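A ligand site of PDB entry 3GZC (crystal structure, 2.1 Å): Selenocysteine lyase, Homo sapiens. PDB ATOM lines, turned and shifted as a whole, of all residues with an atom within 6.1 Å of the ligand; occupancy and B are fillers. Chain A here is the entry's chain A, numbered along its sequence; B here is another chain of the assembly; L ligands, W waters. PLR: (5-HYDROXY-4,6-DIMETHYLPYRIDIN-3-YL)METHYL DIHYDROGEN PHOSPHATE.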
ATOM      1  N   ASN A  32      13.032  16.059 -15.357  1.00  0.00           N
ATOM      2  CA  ASN A  32      13.067  17.520 -15.243  1.00  0.00           C
ATOM      3  C   ASN A  32      11.701  18.082 -14.947  1.00  0.00           C
ATOM      4  O   ASN A  32      11.587  19.133 -14.329  1.00  0.00           O
ATOM      5  CB  ASN A  32      13.670  18.136 -16.507  1.00  0.00           C
ATOM      6  CG  ASN A  32      15.177  18.111 -16.494  1.00  0.00           C
ATOM      7  OD1 ASN A  32      15.795  17.340 -15.738  1.00  0.00           O
ATOM      8  ND2 ASN A  32      15.797  18.924 -17.354  1.00  0.00           N
ATOM      9  N   ALA A  33      10.627  17.368 -15.360  1.00  0.00           N
ATOM     10  CA  ALA A  33       9.262  17.797 -15.082  1.00  0.00           C
ATOM     11  C   ALA A  33       8.902  17.472 -13.617  1.00  0.00           C
ATOM     12  O   ALA A  33       8.320  18.306 -12.905  1.00  0.00           O
ATOM     13  CB  ALA A  33       8.287  17.156 -16.039  1.00  0.00           C
ATOM     14  N   GLY A  93       6.509  25.704  -2.232  1.00  0.00           N
ATOM     15  CA  GLY A  93       7.020  25.242  -3.483  1.00  0.00           C
ATOM     16  C   GLY A  93       7.948  26.254  -4.126  1.00  0.00           C
ATOM     17  O   GLY A  93       8.268  27.297  -3.547  1.00  0.00           O
ATOM     18  N   GLY A  94       8.459  25.900  -5.308  1.00  0.00           N
ATOM     19  CA  GLY A  94       9.344  26.776  -6.049  1.00  0.00           C
ATOM     20  C   GLY A  94       8.707  28.062  -6.517  1.00  0.00           C
ATOM     21  O   GLY A  94       9.333  29.121  -6.482  1.00  0.00           O
ATOM     22  N   THR A  95       7.451  27.999  -6.912  1.00  0.00           N
ATOM     23  CA  THR A  95       6.736  29.160  -7.401  1.00  0.00           C
ATOM     24  C   THR A  95       6.615  30.196  -6.286  1.00  0.00           C
ATOM     25  O   THR A  95       6.850  31.388  -6.530  1.00  0.00           O
ATOM     26  CB  THR A  95       5.345  28.796  -7.918  1.00  0.00           C
ATOM     27  OG1 THR A  95       5.486  27.974  -9.078  1.00  0.00           O
ATOM     28  CG2 THR A  95       4.463  30.062  -8.295  1.00  0.00           C
ATOM     29  N   GLU A  96       6.216  29.738  -5.074  1.00  0.00           N
ATOM     30  CA  GLU A  96       6.116  30.680  -3.927  1.00  0.00           C
ATOM     31  C   GLU A  96       7.498  31.247  -3.602  1.00  0.00           C
ATOM     32  O   GLU A  96       7.613  32.424  -3.354  1.00  0.00           O
ATOM     33  CB  GLU A  96       5.478  30.002  -2.676  1.00  0.00           C
ATOM     34  CG  GLU A  96       5.315  30.966  -1.501  1.00  0.00           C
ATOM     35  CD  GLU A  96       4.857  30.301  -0.225  1.00  0.00           C
ATOM     36  OE1 GLU A  96       5.040  30.942   0.830  1.00  0.00           O
ATOM     37  OE2 GLU A  96       4.359  29.150  -0.269  1.00  0.00           O
ATOM     38  N   ASN A  98      10.134  31.764  -5.486  1.00  0.00           N
ATOM     39  CA  ASN A  98      10.563  32.706  -6.507  1.00  0.00           C
ATOM     40  C   ASN A  98       9.746  33.991  -6.466  1.00  0.00           C
ATOM     41  O   ASN A  98      10.279  35.019  -6.609  1.00  0.00           O
ATOM     42  CB  ASN A  98      10.433  32.111  -7.894  1.00  0.00           C
ATOM     43  CG  ASN A  98      11.577  31.162  -8.282  1.00  0.00           C
ATOM     44  OD1 ASN A  98      12.651  31.163  -7.708  1.00  0.00           O
ATOM     45  ND2 ASN A  98      11.316  30.349  -9.309  1.00  0.00           N
ATOM     46  N   GLU A 139      14.090  32.162 -18.242  1.00  0.00           N
ATOM     47  CA  GLU A 139      13.703  31.794 -16.860  1.00  0.00           C
ATOM     48  C   GLU A 139      12.458  30.944 -16.855  1.00  0.00           C
ATOM     49  O   GLU A 139      11.656  31.006 -17.823  1.00  0.00           O
ATOM     50  CB  GLU A 139      13.453  33.039 -16.025  1.00  0.00           C
ATOM     51  CG  GLU A 139      14.711  33.835 -15.733  1.00  0.00           C
ATOM     52  CD  GLU A 139      15.815  33.095 -14.990  1.00  0.00           C
ATOM     53  OE1 GLU A 139      17.006  33.169 -15.464  1.00  0.00           O
ATOM     54  OE2 GLU A 139      15.499  32.457 -13.933  1.00  0.00           O
ATOM     55  N   HIS A 140      12.307  30.121 -15.815  1.00  0.00           N
ATOM     56  CA  HIS A 140      11.035  29.439 -15.529  1.00  0.00           C
ATOM     57  C   HIS A 140       9.883  30.460 -15.405  1.00  0.00           C
ATOM     58  O   HIS A 140      10.090  31.611 -15.054  1.00  0.00           O
ATOM     59  CB  HIS A 140      11.173  28.515 -14.293  1.00  0.00           C
ATOM     60  CG  HIS A 140       9.957  27.681 -13.981  1.00  0.00           C
ATOM     61  ND1 HIS A 140       8.952  28.130 -13.134  1.00  0.00           N
ATOM     62  CD2 HIS A 140       9.605  26.426 -14.341  1.00  0.00           C
ATOM     63  CE1 HIS A 140       8.013  27.198 -13.036  1.00  0.00           C
ATOM     64  NE2 HIS A 140       8.382  26.161 -13.763  1.00  0.00           N
ATOM     65  N   SER A 142       7.802  30.979 -13.164  1.00  0.00           N
ATOM     66  CA  SER A 142       7.655  31.492 -11.801  1.00  0.00           C
ATOM     67  C   SER A 142       8.641  32.657 -11.518  1.00  0.00           C
ATOM     68  O   SER A 142       8.516  33.340 -10.498  1.00  0.00           O
ATOM     69  CB  SER A 142       7.780  30.344 -10.771  1.00  0.00           C
ATOM     70  OG  SER A 142       9.010  29.696 -10.877  1.00  0.00           O
ATOM     71  N   MET A 189      18.705  31.866 -13.381  1.00  0.00           N
ATOM     72  CA  MET A 189      18.545  30.447 -12.998  1.00  0.00           C
ATOM     73  C   MET A 189      19.849  29.687 -13.004  1.00  0.00           C
ATOM     74  O   MET A 189      20.700  29.967 -13.849  1.00  0.00           O
ATOM     75  CB  MET A 189      17.554  29.760 -13.921  1.00  0.00           C
ATOM     76  CG  MET A 189      18.021  29.603 -15.352  1.00  0.00           C
ATOM     77  SD  MET A 189      16.702  29.380 -16.558  1.00  0.00           S
ATOM     78  CE  MET A 189      15.484  28.303 -15.791  1.00  0.00           C
ATOM     79  N   ALA A 191      20.416  26.334 -13.557  1.00  0.00           N
ATOM     80  CA  ALA A 191      20.339  25.511 -14.759  1.00  0.00           C
ATOM     81  C   ALA A 191      18.986  25.638 -15.397  1.00  0.00           C
ATOM     82  O   ALA A 191      17.983  25.745 -14.719  1.00  0.00           O
ATOM     83  CB  ALA A 191      20.659  24.019 -14.463  1.00  0.00           C
ATOM     84  N   ASN A 192      18.966  25.619 -16.724  1.00  0.00           N
ATOM     85  CA  ASN A 192      17.727  25.767 -17.472  1.00  0.00           C
ATOM     86  C   ASN A 192      17.011  24.436 -17.505  1.00  0.00           C
ATOM     87  O   ASN A 192      17.656  23.396 -17.672  1.00  0.00           O
ATOM     88  CB  ASN A 192      18.016  26.195 -18.877  1.00  0.00           C
ATOM     89  CG  ASN A 192      16.745  26.444 -19.637  1.00  0.00           C
ATOM     90  OD1 ASN A 192      16.379  25.650 -20.448  1.00  0.00           O
ATOM     91  ND2 ASN A 192      16.023  27.512 -19.320  1.00  0.00           N
ATOM     92  N   ASN A 193      15.694  24.459 -17.327  1.00  0.00           N
ATOM     93  CA  ASN A 193      14.926  23.217 -17.259  1.00  0.00           C
ATOM     94  C   ASN A 193      14.778  22.528 -18.583  1.00  0.00           C
ATOM     95  O   ASN A 193      14.641  21.303 -18.618  1.00  0.00           O
ATOM     96  CB  ASN A 193      13.529  23.435 -16.667  1.00  0.00           C
ATOM     97  CG  ASN A 193      12.852  24.688 -17.230  1.00  0.00           C
ATOM     98  OD1 ASN A 193      13.473  25.732 -17.281  1.00  0.00           O
ATOM     99  ND2 ASN A 193      11.603  24.591 -17.610  1.00  0.00           N
ATOM    100  N   ASP A 228      17.556  30.603  -9.061  1.00  0.00           N
ATOM    101  CA  ASP A 228      16.564  29.551  -9.013  1.00  0.00           C
ATOM    102  C   ASP A 228      17.344  28.265  -9.313  1.00  0.00           C
ATOM    103  O   ASP A 228      17.704  28.001 -10.439  1.00  0.00           O
ATOM    104  CB  ASP A 228      15.469  29.849 -10.014  1.00  0.00           C
ATOM    105  CG  ASP A 228      14.455  28.774 -10.095  1.00  0.00           C
ATOM    106  OD1 ASP A 228      13.449  29.000 -10.802  1.00  0.00           O
ATOM    107  OD2 ASP A 228      14.688  27.702  -9.479  1.00  0.00           O
ATOM    108  N   ALA A 230      16.283  25.232  -8.886  1.00  0.00           N
ATOM    109  CA  ALA A 230      15.297  24.136  -8.947  1.00  0.00           C
ATOM    110  C   ALA A 230      15.851  22.932  -9.698  1.00  0.00           C
ATOM    111  O   ALA A 230      15.729  21.787  -9.228  1.00  0.00           O
ATOM    112  CB  ALA A 230      14.020  24.577  -9.565  1.00  0.00           C
ATOM    113  N   GLN A 231      16.498  23.174 -10.833  1.00  0.00           N
ATOM    114  CA  GLN A 231      16.925  22.033 -11.684  1.00  0.00           C
ATOM    115  C   GLN A 231      18.250  21.427 -11.370  1.00  0.00           C
ATOM    116  O   GLN A 231      18.552  20.351 -11.894  1.00  0.00           O
ATOM    117  CB  GLN A 231      16.890  22.423 -13.164  1.00  0.00           C
ATOM    118  CG  GLN A 231      15.459  22.540 -13.670  1.00  0.00           C
ATOM    119  CD  GLN A 231      14.748  21.238 -13.815  1.00  0.00           C
ATOM    120  OE1 GLN A 231      15.366  20.174 -13.836  1.00  0.00           O
ATOM    121  NE2 GLN A 231      13.424  21.301 -13.957  1.00  0.00           N
ATOM    122  N   THR A 249      16.420  29.370  -4.498  1.00  0.00           N
ATOM    123  CA  THR A 249      15.201  28.568  -4.518  1.00  0.00           C
ATOM    124  C   THR A 249      15.444  27.049  -4.613  1.00  0.00           C
ATOM    125  O   THR A 249      16.172  26.554  -5.507  1.00  0.00           O
ATOM    126  CB  THR A 249      14.274  28.977  -5.689  1.00  0.00           C
ATOM    127  OG1 THR A 249      13.915  30.378  -5.500  1.00  0.00           O
ATOM    128  CG2 THR A 249      13.029  28.070  -5.760  1.00  0.00           C
ATOM    129  N   VAL A 251      13.486  23.264  -4.638  1.00  0.00           N
ATOM    130  CA  VAL A 251      12.264  22.663  -5.189  1.00  0.00           C
ATOM    131  C   VAL A 251      12.296  21.134  -4.976  1.00  0.00           C
ATOM    132  O   VAL A 251      12.957  20.400  -5.711  1.00  0.00           O
ATOM    133  CB  VAL A 251      12.029  23.044  -6.684  1.00  0.00           C
ATOM    134  CG1 VAL A 251      10.616  22.703  -7.109  1.00  0.00           C
ATOM    135  CG2 VAL A 251      12.199  24.480  -6.869  1.00  0.00           C
ATOM    136  N   HIS A 253      10.364  18.557  -5.398  1.00  0.00           N
ATOM    137  CA  HIS A 253       9.891  17.563  -6.344  1.00  0.00           C
ATOM    138  C   HIS A 253      10.822  17.441  -7.540  1.00  0.00           C
ATOM    139  O   HIS A 253      10.557  16.640  -8.395  1.00  0.00           O
ATOM    140  CB  HIS A 253       8.424  17.777  -6.707  1.00  0.00           C
ATOM    141  CG  HIS A 253       8.158  18.867  -7.723  1.00  0.00           C
ATOM    142  ND1 HIS A 253       7.865  18.587  -9.046  1.00  0.00           N
ATOM    143  CD2 HIS A 253       8.094  20.229  -7.616  1.00  0.00           C
ATOM    144  CE1 HIS A 253       7.627  19.713  -9.698  1.00  0.00           C
ATOM    145  NE2 HIS A 253       7.765  20.722  -8.855  1.00  0.00           N
ATOM    146  N   LYS A 254      11.904  18.217  -7.577  1.00  0.00           N
ATOM    147  CA  LYS A 254      12.973  18.009  -8.559  1.00  0.00           C
ATOM    148  C   LYS A 254      14.101  17.101  -8.073  1.00  0.00           C
ATOM    149  O   LYS A 254      14.864  16.616  -8.869  1.00  0.00           O
ATOM    150  CB  LYS A 254      13.478  19.354  -9.066  1.00  0.00           C
ATOM    151  CG  LYS A 254      12.353  20.283  -9.573  1.00  0.00           C
ATOM    152  CD  LYS A 254      11.849  19.846 -10.889  1.00  0.00           C
ATOM    153  CE  LYS A 254      10.703  20.720 -11.462  1.00  0.00           C
ATOM    154  NZ  LYS A 254      10.941  22.131 -11.551  1.00  0.00           N
ATOM    155  N   ARG A 259       6.184  17.908  -2.862  1.00  0.00           N
ATOM    156  CA  ARG A 259       5.874  19.118  -3.605  1.00  0.00           C
ATOM    157  C   ARG A 259       5.854  20.401  -2.764  1.00  0.00           C
ATOM    158  O   ARG A 259       4.975  21.281  -2.931  1.00  0.00           O
ATOM    159  CB  ARG A 259       4.542  18.926  -4.377  1.00  0.00           C
ATOM    160  CG  ARG A 259       4.641  17.856  -5.477  1.00  0.00           C
ATOM    161  CD  ARG A 259       4.621  18.447  -6.873  1.00  0.00           C
ATOM    162  NE  ARG A 259       4.976  17.396  -7.828  1.00  0.00           N
ATOM    163  CZ  ARG A 259       4.153  16.477  -8.334  1.00  0.00           C
ATOM    164  NH1 ARG A 259       2.864  16.458  -8.043  1.00  0.00           N
ATOM    165  NH2 ARG A 259       4.635  15.543  -9.147  1.00  0.00           N
ATOM    166  N   GLN B 283      -1.286  26.715 -13.258  1.00  0.00           N
ATOM    167  CA  GLN B 283      -2.065  25.707 -12.498  1.00  0.00           C
ATOM    168  C   GLN B 283      -3.204  26.375 -11.682  1.00  0.00           C
ATOM    169  O   GLN B 283      -3.151  27.575 -11.311  1.00  0.00           O
ATOM    170  CB  GLN B 283      -1.194  24.906 -11.567  1.00  0.00           C
ATOM    171  CG  GLN B 283      -0.113  24.023 -12.212  1.00  0.00           C
ATOM    172  CD  GLN B 283       1.191  24.738 -12.372  1.00  0.00           C
ATOM    173  OE1 GLN B 283       1.256  25.951 -12.255  1.00  0.00           O
ATOM    174  NE2 GLN B 283       2.243  24.000 -12.660  1.00  0.00           N
ATOM    175  N   PRO B 289      -0.964  29.283  -9.249  1.00  0.00           N
ATOM    176  CA  PRO B 289      -0.025  28.452  -9.983  1.00  0.00           C
ATOM    177  C   PRO B 289       1.001  27.793  -9.056  1.00  0.00           C
ATOM    178  O   PRO B 289       1.061  28.107  -7.837  1.00  0.00           O
ATOM    179  CB  PRO B 289       0.627  29.439 -10.963  1.00  0.00           C
ATOM    180  CG  PRO B 289       0.310  30.732 -10.512  1.00  0.00           C
ATOM    181  CD  PRO B 289      -0.609  30.702  -9.329  1.00  0.00           C
ATOM    182  N   GLY B 290       1.781  26.876  -9.608  1.00  0.00           N
ATOM    183  CA  GLY B 290       2.676  26.031  -8.849  1.00  0.00           C
ATOM    184  C   GLY B 290       2.217  24.581  -9.010  1.00  0.00           C
ATOM    185  O   GLY B 290       1.015  24.310  -8.949  1.00  0.00           O
ATOM    186  N   THR B 291       3.140  23.647  -9.227  1.00  0.00           N
ATOM    187  CA  THR B 291       2.793  22.232  -9.406  1.00  0.00           C
ATOM    188  C   THR B 291       1.991  21.703  -8.235  1.00  0.00           C
ATOM    189  O   THR B 291       2.307  22.003  -7.116  1.00  0.00           O
ATOM    190  CB  THR B 291       4.072  21.357  -9.571  1.00  0.00           C
ATOM    191  OG1 THR B 291       4.873  21.925 -10.604  1.00  0.00           O
ATOM    192  CG2 THR B 291       3.751  19.938  -9.981  1.00  0.00           C
HETATM  193  N1  PLR L   1      12.136  26.866 -11.542  1.00  0.00           N
HETATM  194  C2  PLR L   1      12.534  25.901 -12.392  1.00  0.00           C
HETATM  195  C2A PLR L   1      13.680  26.230 -13.307  1.00  0.00           C
HETATM  196  C3  PLR L   1      11.855  24.673 -12.352  1.00  0.00           C
HETATM  197  O3  PLR L   1      12.195  23.649 -13.182  1.00  0.00           O
HETATM  198  C4  PLR L   1      10.830  24.492 -11.430  1.00  0.00           C
HETATM  199  C4A PLR L   1      10.136  23.181 -11.375  1.00  0.00           C
HETATM  200  C5  PLR L   1      10.477  25.558 -10.578  1.00  0.00           C
HETATM  201  C6  PLR L   1      11.180  26.721 -10.675  1.00  0.00           C
HETATM  202  C5A PLR L   1       9.373  25.497  -9.547  1.00  0.00           C
HETATM  203  O4P PLR L   1       8.086  25.230 -10.105  1.00  0.00           O
HETATM  204  P   PLR L   1       6.881  24.565  -9.252  1.00  0.00           P
HETATM  205  O1P PLR L   1       7.409  23.354  -8.586  1.00  0.00           O
HETATM  206  O2P PLR L   1       6.349  25.525  -8.212  1.00  0.00           O
HETATM  207  O3P PLR L   1       5.877  24.358 -10.355  1.00  0.00           O
HETATM  208  O   HOH W   1       5.019  25.230 -12.704  1.00  0.00           O
HETATM  209  O   HOH W   2       7.278  23.074  -6.062  1.00  0.00           O
HETATM  210  O   HOH W   3       4.629  25.211  -6.194  1.00  0.00           O
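N of Thr 291 of chain B lies within hydrogen-bond range of O3P of the ligand, 3.0 Å away.
OD1 of Asp 228 lies within hydrogen-bond range of N1 of the ligand (2.6 Å).
The backbone NH (N) of Thr 95 sits at hydrogen-bond distance from an oxygen (O2P) of the ligand, at 3.0 Å.
The side-chain amino group of Lys 254 is bonded to a carbon (C4A) of the ligand (1.3 Å).
A ring nitrogen (NE2) of His 253 lies within hydrogen-bond range of an oxygen (O1P) of the ligand (2.7 Å).
The side-chain hydroxyl of Thr 95 sits at hydrogen-bond distance from an oxygen (O2P) of the ligand.
The side-chain amide nitrogen of Gln 231 lies within hydrogen-bond range of an oxygen (O3) of the ligand.
The side-chain hydroxyl (OG1) of Thr 291 of chain B sits at hydrogen-bond distance from an oxygen (O3P) of the ligand (2.6 Å).
The side-chain hydroxyl (OG) of Ser 142 lies within hydrogen-bond range of a ring nitrogen (ND1) of His 140, 2.7 Å away.
The side-chain carboxylate of Asp 228 is in hydrogen-bond range of the backbone NH of Ala 230, at 3.0 Å.
The backbone carbonyl oxygen of Asn 32 sits at hydrogen-bond distance from the side-chain amide nitrogen of Gln 231 (2.9 Å).
OG of Ser 142 is in hydrogen-bond range of ND2 of Asn 98, 2.9 Å away.
N of Met 189 is in hydrogen-bond range of OE1 of Glu 139, at 3.0 Å.
The side-chain amide nitrogen (ND2) of Asn 32 is in hydrogen-bond range of the backbone carbonyl oxygen (O) of Asn 193 (2.9 Å).
ND1 of His 253 lies within hydrogen-bond range of NE of Arg 259 (3.4 Å).
The side-chain sulfur of Met 189 is in hydrogen-bond range of the side-chain amide nitrogen of Asn 192.
Merely in contact with the ligand: Gly 94 (3.6 Å), Asn 98 (3.9 Å), His 140 (3.3 Å), Ser 142 (3.7 Å), Met 189 (3.7 Å), Asn 193 (3.7 Å), Ala 230 (3.5 Å), Val 251 (3.6 Å) and Gly 290 of chain B (3.8 Å).
Hydrophobic or aromatic side chains within 4 Å of the ligand: His 140, Met 189, Ala 230, Val 251 and His 253.
Of the 26 residues printed, 15 come within 4 Å of the ligand.
Along chain A the residues within 4 Å of the ligand span positions 94 to 254.
The nearest printed residue that does not touch the ligand is Gln 283 of chain B (4.3 Å).
Water W2 bridges O1P of the ligand (2.5 Å) and N of Gly 94 (3.2 Å).
Water W1 lies within hydrogen-bond range of O3P of the ligand and NE2 of Gln 283 of chain B.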
